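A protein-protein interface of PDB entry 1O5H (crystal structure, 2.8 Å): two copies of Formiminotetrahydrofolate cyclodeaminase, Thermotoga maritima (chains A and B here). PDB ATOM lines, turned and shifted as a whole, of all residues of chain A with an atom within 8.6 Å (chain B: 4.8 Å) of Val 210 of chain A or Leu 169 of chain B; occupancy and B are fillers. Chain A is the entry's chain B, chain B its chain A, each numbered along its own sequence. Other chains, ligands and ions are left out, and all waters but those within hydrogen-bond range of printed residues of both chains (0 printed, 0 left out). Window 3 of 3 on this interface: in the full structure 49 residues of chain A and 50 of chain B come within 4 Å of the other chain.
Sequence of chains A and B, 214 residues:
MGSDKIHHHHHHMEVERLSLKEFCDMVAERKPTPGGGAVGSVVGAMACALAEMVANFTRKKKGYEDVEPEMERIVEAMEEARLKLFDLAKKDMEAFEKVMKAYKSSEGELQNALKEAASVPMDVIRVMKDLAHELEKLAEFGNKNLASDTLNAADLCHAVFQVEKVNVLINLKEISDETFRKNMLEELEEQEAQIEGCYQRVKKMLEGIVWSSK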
ATOM      1  N   ALA A 147       8.855  11.216  -2.753  1.00  0.00           N
ATOM      2  CA  ALA A 147       7.856  10.588  -3.581  1.00  0.00           C
ATOM      3  C   ALA A 147       7.128   9.511  -2.792  1.00  0.00           C
ATOM      4  O   ALA A 147       5.897   9.434  -2.826  1.00  0.00           O
ATOM      5  CB  ALA A 147       8.471  10.027  -4.845  1.00  0.00           C
ATOM      6  N   SER A 148       7.882   8.707  -2.047  1.00  0.00           N
ATOM      7  CA  SER A 148       7.276   7.634  -1.258  1.00  0.00           C
ATOM      8  C   SER A 148       6.142   8.187  -0.415  1.00  0.00           C
ATOM      9  O   SER A 148       5.059   7.613  -0.371  1.00  0.00           O
ATOM     10  CB  SER A 148       8.308   7.013  -0.350  1.00  0.00           C
ATOM     11  OG  SER A 148       8.114   7.511   0.954  1.00  0.00           O
ATOM     12  N   LEU A 151       3.215   9.016  -2.464  1.00  0.00           N
ATOM     13  CA  LEU A 151       2.491   7.834  -2.903  1.00  0.00           C
ATOM     14  C   LEU A 151       1.704   7.281  -1.745  1.00  0.00           C
ATOM     15  O   LEU A 151       0.528   6.916  -1.897  1.00  0.00           O
ATOM     16  CB  LEU A 151       3.429   6.753  -3.367  1.00  0.00           C
ATOM     17  CG  LEU A 151       3.321   6.284  -4.799  1.00  0.00           C
ATOM     18  CD1 LEU A 151       4.326   5.164  -4.981  1.00  0.00           C
ATOM     19  CD2 LEU A 151       1.884   5.830  -5.092  1.00  0.00           C
ATOM     20  N   ASN A 152       2.331   7.220  -0.576  1.00  0.00           N
ATOM     21  CA  ASN A 152       1.617   6.751   0.565  1.00  0.00           C
ATOM     22  C   ASN A 152       0.379   7.577   0.714  1.00  0.00           C
ATOM     23  O   ASN A 152      -0.677   7.035   0.949  1.00  0.00           O
ATOM     24  CB  ASN A 152       2.466   6.881   1.810  1.00  0.00           C
ATOM     25  CG  ASN A 152       3.609   5.916   1.815  1.00  0.00           C
ATOM     26  OD1 ASN A 152       3.707   5.037   0.950  1.00  0.00           O
ATOM     27  ND2 ASN A 152       4.466   6.032   2.808  1.00  0.00           N
ATOM     28  N   MET A 205       3.017   8.297 -12.437  1.00  0.00           N
ATOM     29  CA  MET A 205       4.162   9.163 -12.323  1.00  0.00           C
ATOM     30  C   MET A 205       5.146   8.664 -11.297  1.00  0.00           C
ATOM     31  O   MET A 205       6.325   8.843 -11.446  1.00  0.00           O
ATOM     32  CB  MET A 205       3.677  10.518 -11.873  1.00  0.00           C
ATOM     33  CG  MET A 205       4.333  11.711 -12.524  1.00  0.00           C
ATOM     34  SD  MET A 205       3.190  13.351 -12.310  1.00  0.00           S
ATOM     35  CE  MET A 205       1.438  12.633 -13.009  1.00  0.00           C
ATOM     36  N   LEU A 206       4.682   8.029 -10.244  1.00  0.00           N
ATOM     37  CA  LEU A 206       5.576   7.756  -9.123  1.00  0.00           C
ATOM     38  C   LEU A 206       5.929   6.302  -8.886  1.00  0.00           C
ATOM     39  O   LEU A 206       6.821   6.036  -8.098  1.00  0.00           O
ATOM     40  CB  LEU A 206       4.988   8.308  -7.827  1.00  0.00           C
ATOM     41  CG  LEU A 206       4.954   9.810  -7.688  1.00  0.00           C
ATOM     42  CD1 LEU A 206       4.851  10.181  -6.196  1.00  0.00           C
ATOM     43  CD2 LEU A 206       6.179  10.436  -8.324  1.00  0.00           C
ATOM     44  N   GLU A 207       5.218   5.369  -9.509  1.00  0.00           N
ATOM     45  CA  GLU A 207       5.495   3.943  -9.311  1.00  0.00           C
ATOM     46  C   GLU A 207       6.992   3.564  -9.408  1.00  0.00           C
ATOM     47  O   GLU A 207       7.420   2.668  -8.690  1.00  0.00           O
ATOM     48  CB  GLU A 207       4.621   3.062 -10.241  1.00  0.00           C
ATOM     49  N   GLY A 208       7.770   4.259 -10.258  1.00  0.00           N
ATOM     50  CA  GLY A 208       9.200   3.968 -10.509  1.00  0.00           C
ATOM     51  C   GLY A 208      10.203   4.209  -9.387  1.00  0.00           C
ATOM     52  O   GLY A 208      11.334   3.735  -9.438  1.00  0.00           O
ATOM     53  N   ILE A 209       9.801   4.945  -8.366  1.00  0.00           N
ATOM     54  CA  ILE A 209      10.644   5.186  -7.202  1.00  0.00           C
ATOM     55  C   ILE A 209      10.850   3.916  -6.383  1.00  0.00           C
ATOM     56  O   ILE A 209      11.751   3.838  -5.548  1.00  0.00           O
ATOM     57  CB  ILE A 209       9.956   6.195  -6.323  1.00  0.00           C
ATOM     58  CG1 ILE A 209       8.772   5.507  -5.570  1.00  0.00           C
ATOM     59  CG2 ILE A 209       9.572   7.422  -7.197  1.00  0.00           C
ATOM     60  CD1 ILE A 209       8.334   6.170  -4.286  1.00  0.00           C
ATOM     61  N   VAL A 210       9.998   2.930  -6.627  1.00  0.00           N
ATOM     62  CA  VAL A 210      10.023   1.671  -5.911  1.00  0.00           C
ATOM     63  C   VAL A 210      11.206   0.752  -6.289  1.00  0.00           C
ATOM     64  O   VAL A 210      11.502  -0.227  -5.585  1.00  0.00           O
ATOM     65  CB  VAL A 210       8.632   0.979  -6.033  1.00  0.00           C
ATOM     66  CG1 VAL A 210       8.707  -0.387  -6.739  1.00  0.00           C
ATOM     67  CG2 VAL A 210       7.933   0.917  -4.680  1.00  0.00           C
ATOM     68  N   TRP A 211      11.890   1.079  -7.384  1.00  0.00           N
ATOM     69  CA  TRP A 211      13.148   0.401  -7.746  1.00  0.00           C
ATOM     70  C   TRP A 211      14.243   1.391  -8.121  1.00  0.00           C
ATOM     71  O   TRP A 211      15.404   1.010  -8.208  1.00  0.00           O
ATOM     72  CB  TRP A 211      12.931  -0.618  -8.871  1.00  0.00           C
ATOM     73  CG  TRP A 211      12.335  -0.014 -10.095  1.00  0.00           C
ATOM     74  CD1 TRP A 211      12.994   0.716 -11.047  1.00  0.00           C
ATOM     75  CD2 TRP A 211      10.955  -0.056 -10.504  1.00  0.00           C
ATOM     76  NE1 TRP A 211      12.116   1.124 -12.022  1.00  0.00           N
ATOM     77  CE2 TRP A 211      10.858   0.664 -11.722  1.00  0.00           C
ATOM     78  CE3 TRP A 211       9.784  -0.632  -9.968  1.00  0.00           C
ATOM     79  CZ2 TRP A 211       9.638   0.824 -12.419  1.00  0.00           C
ATOM     80  CZ3 TRP A 211       8.563  -0.476 -10.662  1.00  0.00           C
ATOM     81  CH2 TRP A 211       8.506   0.246 -11.875  1.00  0.00           C
ATOM     82  N   LYS B 165       4.242  -1.543   1.775  1.00  0.00           N
ATOM     83  CA  LYS B 165       4.977  -2.179   0.694  1.00  0.00           C
ATOM     84  C   LYS B 165       5.940  -1.179   0.108  1.00  0.00           C
ATOM     85  O   LYS B 165       7.149  -1.488  -0.052  1.00  0.00           O
ATOM     86  CB  LYS B 165       4.048  -2.635  -0.408  1.00  0.00           C
ATOM     87  CG  LYS B 165       4.748  -3.272  -1.564  1.00  0.00           C
ATOM     88  CD  LYS B 165       3.755  -3.656  -2.646  1.00  0.00           C
ATOM     89  CE  LYS B 165       4.454  -4.445  -3.733  1.00  0.00           C
ATOM     90  NZ  LYS B 165       3.471  -4.747  -4.773  1.00  0.00           N
ATOM     91  N   VAL B 166       5.447   0.022  -0.195  1.00  0.00           N
ATOM     92  CA  VAL B 166       6.367   1.039  -0.679  1.00  0.00           C
ATOM     93  C   VAL B 166       7.529   1.255   0.311  1.00  0.00           C
ATOM     94  O   VAL B 166       8.705   1.326  -0.092  1.00  0.00           O
ATOM     95  CB  VAL B 166       5.655   2.341  -1.035  1.00  0.00           C
ATOM     96  CG1 VAL B 166       6.620   3.547  -0.997  1.00  0.00           C
ATOM     97  CG2 VAL B 166       5.016   2.203  -2.402  1.00  0.00           C
ATOM     98  N   ASN B 167       7.216   1.313   1.601  1.00  0.00           N
ATOM     99  CA  ASN B 167       8.267   1.537   2.564  1.00  0.00           C
ATOM    100  C   ASN B 167       9.242   0.368   2.684  1.00  0.00           C
ATOM    101  O   ASN B 167      10.460   0.578   2.791  1.00  0.00           O
ATOM    102  CB  ASN B 167       7.692   2.021   3.886  1.00  0.00           C
ATOM    103  CG  ASN B 167       7.056   3.394   3.757  1.00  0.00           C
ATOM    104  OD1 ASN B 167       5.956   3.623   4.233  1.00  0.00           O
ATOM    105  ND2 ASN B 167       7.736   4.305   3.079  1.00  0.00           N
ATOM    106  N   VAL B 168       8.734  -0.858   2.602  1.00  0.00           N
ATOM    107  CA  VAL B 168       9.633  -2.009   2.463  1.00  0.00           C
ATOM    108  C   VAL B 168      10.565  -1.876   1.253  1.00  0.00           C
ATOM    109  O   VAL B 168      11.786  -2.030   1.385  1.00  0.00           O
ATOM    110  CB  VAL B 168       8.882  -3.323   2.384  1.00  0.00           C
ATOM    111  CG1 VAL B 168       9.798  -4.427   1.893  1.00  0.00           C
ATOM    112  CG2 VAL B 168       8.359  -3.662   3.740  1.00  0.00           C
ATOM    113  N   LEU B 169      10.013  -1.570   0.080  1.00  0.00           N
ATOM    114  CA  LEU B 169      10.879  -1.496  -1.097  1.00  0.00           C
ATOM    115  C   LEU B 169      11.864  -0.338  -1.104  1.00  0.00           C
ATOM    116  O   LEU B 169      12.998  -0.531  -1.538  1.00  0.00           O
ATOM    117  CB  LEU B 169      10.104  -1.541  -2.391  1.00  0.00           C
ATOM    118  CG  LEU B 169       9.242  -2.787  -2.510  1.00  0.00           C
ATOM    119  CD1 LEU B 169       8.544  -2.801  -3.840  1.00  0.00           C
ATOM    120  CD2 LEU B 169      10.074  -4.013  -2.362  1.00  0.00           C
ATOM    121  N   ILE B 170      11.472   0.844  -0.627  1.00  0.00           N
ATOM    122  CA  ILE B 170      12.456   1.934  -0.595  1.00  0.00           C
ATOM    123  C   ILE B 170      13.662   1.519   0.218  1.00  0.00           C
ATOM    124  O   ILE B 170      14.782   1.859  -0.139  1.00  0.00           O
ATOM    125  CB  ILE B 170      11.901   3.316  -0.122  1.00  0.00           C
ATOM    126  CG1 ILE B 170      11.289   3.214   1.294  1.00  0.00           C
ATOM    127  CG2 ILE B 170      10.979   3.923  -1.216  1.00  0.00           C
ATOM    128  CD1 ILE B 170      11.059   4.554   2.054  1.00  0.00           C
ATOM    129  N   ASN B 171      13.451   0.759   1.287  1.00  0.00           N
ATOM    130  CA  ASN B 171      14.571   0.300   2.080  1.00  0.00           C
ATOM    131  C   ASN B 171      15.403  -0.794   1.447  1.00  0.00           C
ATOM    132  O   ASN B 171      16.637  -0.689   1.374  1.00  0.00           O
ATOM    133  CB  ASN B 171      14.092  -0.087   3.439  1.00  0.00           C
ATOM    134  CG  ASN B 171      13.750   1.116   4.268  1.00  0.00           C
ATOM    135  OD1 ASN B 171      14.632   1.733   4.871  1.00  0.00           O
ATOM    136  ND2 ASN B 171      12.491   1.482   4.286  1.00  0.00           N
ATOM    137  N   LEU B 172      14.737  -1.815   0.939  1.00  0.00           N
ATOM    138  CA  LEU B 172      15.441  -2.902   0.278  1.00  0.00           C
ATOM    139  C   LEU B 172      16.459  -2.461  -0.756  1.00  0.00           C
ATOM    140  O   LEU B 172      17.565  -3.011  -0.798  1.00  0.00           O
ATOM    141  CB  LEU B 172      14.452  -3.853  -0.381  1.00  0.00           C
ATOM    142  CG  LEU B 172      13.752  -4.736   0.638  1.00  0.00           C
ATOM    143  CD1 LEU B 172      12.993  -5.801  -0.082  1.00  0.00           C
ATOM    144  CD2 LEU B 172      14.786  -5.333   1.581  1.00  0.00           C
ATOM    145  N   LYS B 173      16.087  -1.482  -1.587  1.00  0.00           N
ATOM    146  CA  LYS B 173      16.918  -1.066  -2.719  1.00  0.00           C
ATOM    147  C   LYS B 173      18.279  -0.541  -2.295  1.00  0.00           C
ATOM    148  O   LYS B 173      19.218  -0.520  -3.084  1.00  0.00           O
ATOM    149  CB  LYS B 173      16.203  -0.060  -3.613  1.00  0.00           C
ATOM    150  CG  LYS B 173      16.028   1.311  -3.014  1.00  0.00           C
ATOM    151  CD  LYS B 173      15.333   2.244  -4.004  1.00  0.00           C
ATOM    152  CE  LYS B 173      14.945   3.545  -3.307  1.00  0.00           C
ATOM    153  NZ  LYS B 173      14.788   4.686  -4.252  1.00  0.00           N
ATOM    154  N   LEU B 185      11.711  -9.928  -0.245  1.00  0.00           N
ATOM    155  CA  LEU B 185      10.859  -9.757  -1.397  1.00  0.00           C
ATOM    156  C   LEU B 185       9.902 -10.913  -1.487  1.00  0.00           C
ATOM    157  O   LEU B 185       8.711 -10.742  -1.754  1.00  0.00           O
ATOM    158  CB  LEU B 185      11.688  -9.669  -2.663  1.00  0.00           C
ATOM    159  CG  LEU B 185      11.871  -8.291  -3.305  1.00  0.00           C
ATOM    160  CD1 LEU B 185      12.664  -7.458  -2.411  1.00  0.00           C
ATOM    161  CD2 LEU B 185      12.659  -8.451  -4.556  1.00  0.00           C
ATOM    162  N   LEU B 188       7.268 -10.572   1.236  1.00  0.00           N
ATOM    163  CA  LEU B 188       6.372  -9.539   0.758  1.00  0.00           C
ATOM    164  C   LEU B 188       5.363 -10.097  -0.255  1.00  0.00           C
ATOM    165  O   LEU B 188       4.190  -9.781  -0.213  1.00  0.00           O
ATOM    166  CB  LEU B 188       7.190  -8.439   0.126  1.00  0.00           C
ATOM    167  CG  LEU B 188       6.432  -7.320  -0.523  1.00  0.00           C
ATOM    168  CD1 LEU B 188       5.386  -6.785   0.435  1.00  0.00           C
ATOM    169  CD2 LEU B 188       7.435  -6.228  -0.906  1.00  0.00           C
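Of chain B, only Val 166 (3.9 Å) and Leu 169 (3.7 Å) come within 4 Å of Val 210 of chain A.
Val 168 of chain B touches none of the printed residues of chain A.
Printed residues of chain A within 4 Å of Lys 173 of chain B: Ile 209.
Of the printed residues of chain B, Leu 151 of chain A touches Val 166.
Printed residues of chain A within 4 Å of Val 166 of chain B: Ser 148, Leu 151, Asn 152 and Val 210.
Printed residues of chain B within 4 Å of Ser 148 of chain A: Val 166 and Asn 167.
The nearest residue of chain A that does not touch Leu 169 of chain B is Trp 211 of chain A (5.9 Å).
The nearest printed residue of chain B that does not touch Ile 209 of chain A is Ile 170 of chain B (4.4 Å).
O of Ser 148 of chain A sits close to OD1 of Asn 152 of chain A, at 3.2 Å.
ND2 of Asn 171 of chain B sits at hydrogen-bond distance from O of Asn 167 of chain B, 2.7 Å away.
Of the 11 printed residues of chain B, 4 touch a printed residue of chain A.
Hydrophobic or aromatic side chains of chain B that line the printed part of chain A: Val 166 and Leu 169.
Among the printed residues, 8 pairs touch across the chains.
Among the printed residues, no Asp or Glu carboxylate lies within 4 Å of a Lys or Arg side-chain nitrogen of the other chain.
No position is printed for both chains.
Of the 8 pairs that touch across the chains among the printed residues, none has its exchanged pair printed and touching as well.
Val 166 of chain B touches Ser 148 of chain A.
ND2 of Asn 167 of chain B touches OG of Ser 148 of chain A, at 3.9 Å.
Val 166 of chain B touches Leu 151 of chain A.
Asn 152 of chain A touches Val 166 of chain B (OD1 to CG1, 3.8 Å).
CG2 of Val 166 of chain B touches CG2 of Val 210 of chain A (3.9 Å).
CB of Leu 169 of chain B touches O of Val 210 of chain A, at 3.7 Å.
ND2 of Asn 152 of chain A sits at hydrogen-bond distance from OD1 of Asn 167 of chain B, at 3.2 Å.
The side-chain amino group (NZ) of Lys 173 of chain B lies within hydrogen-bond range of the backbone carbonyl oxygen (O) of Ile 209 of chain A (3.4 Å).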
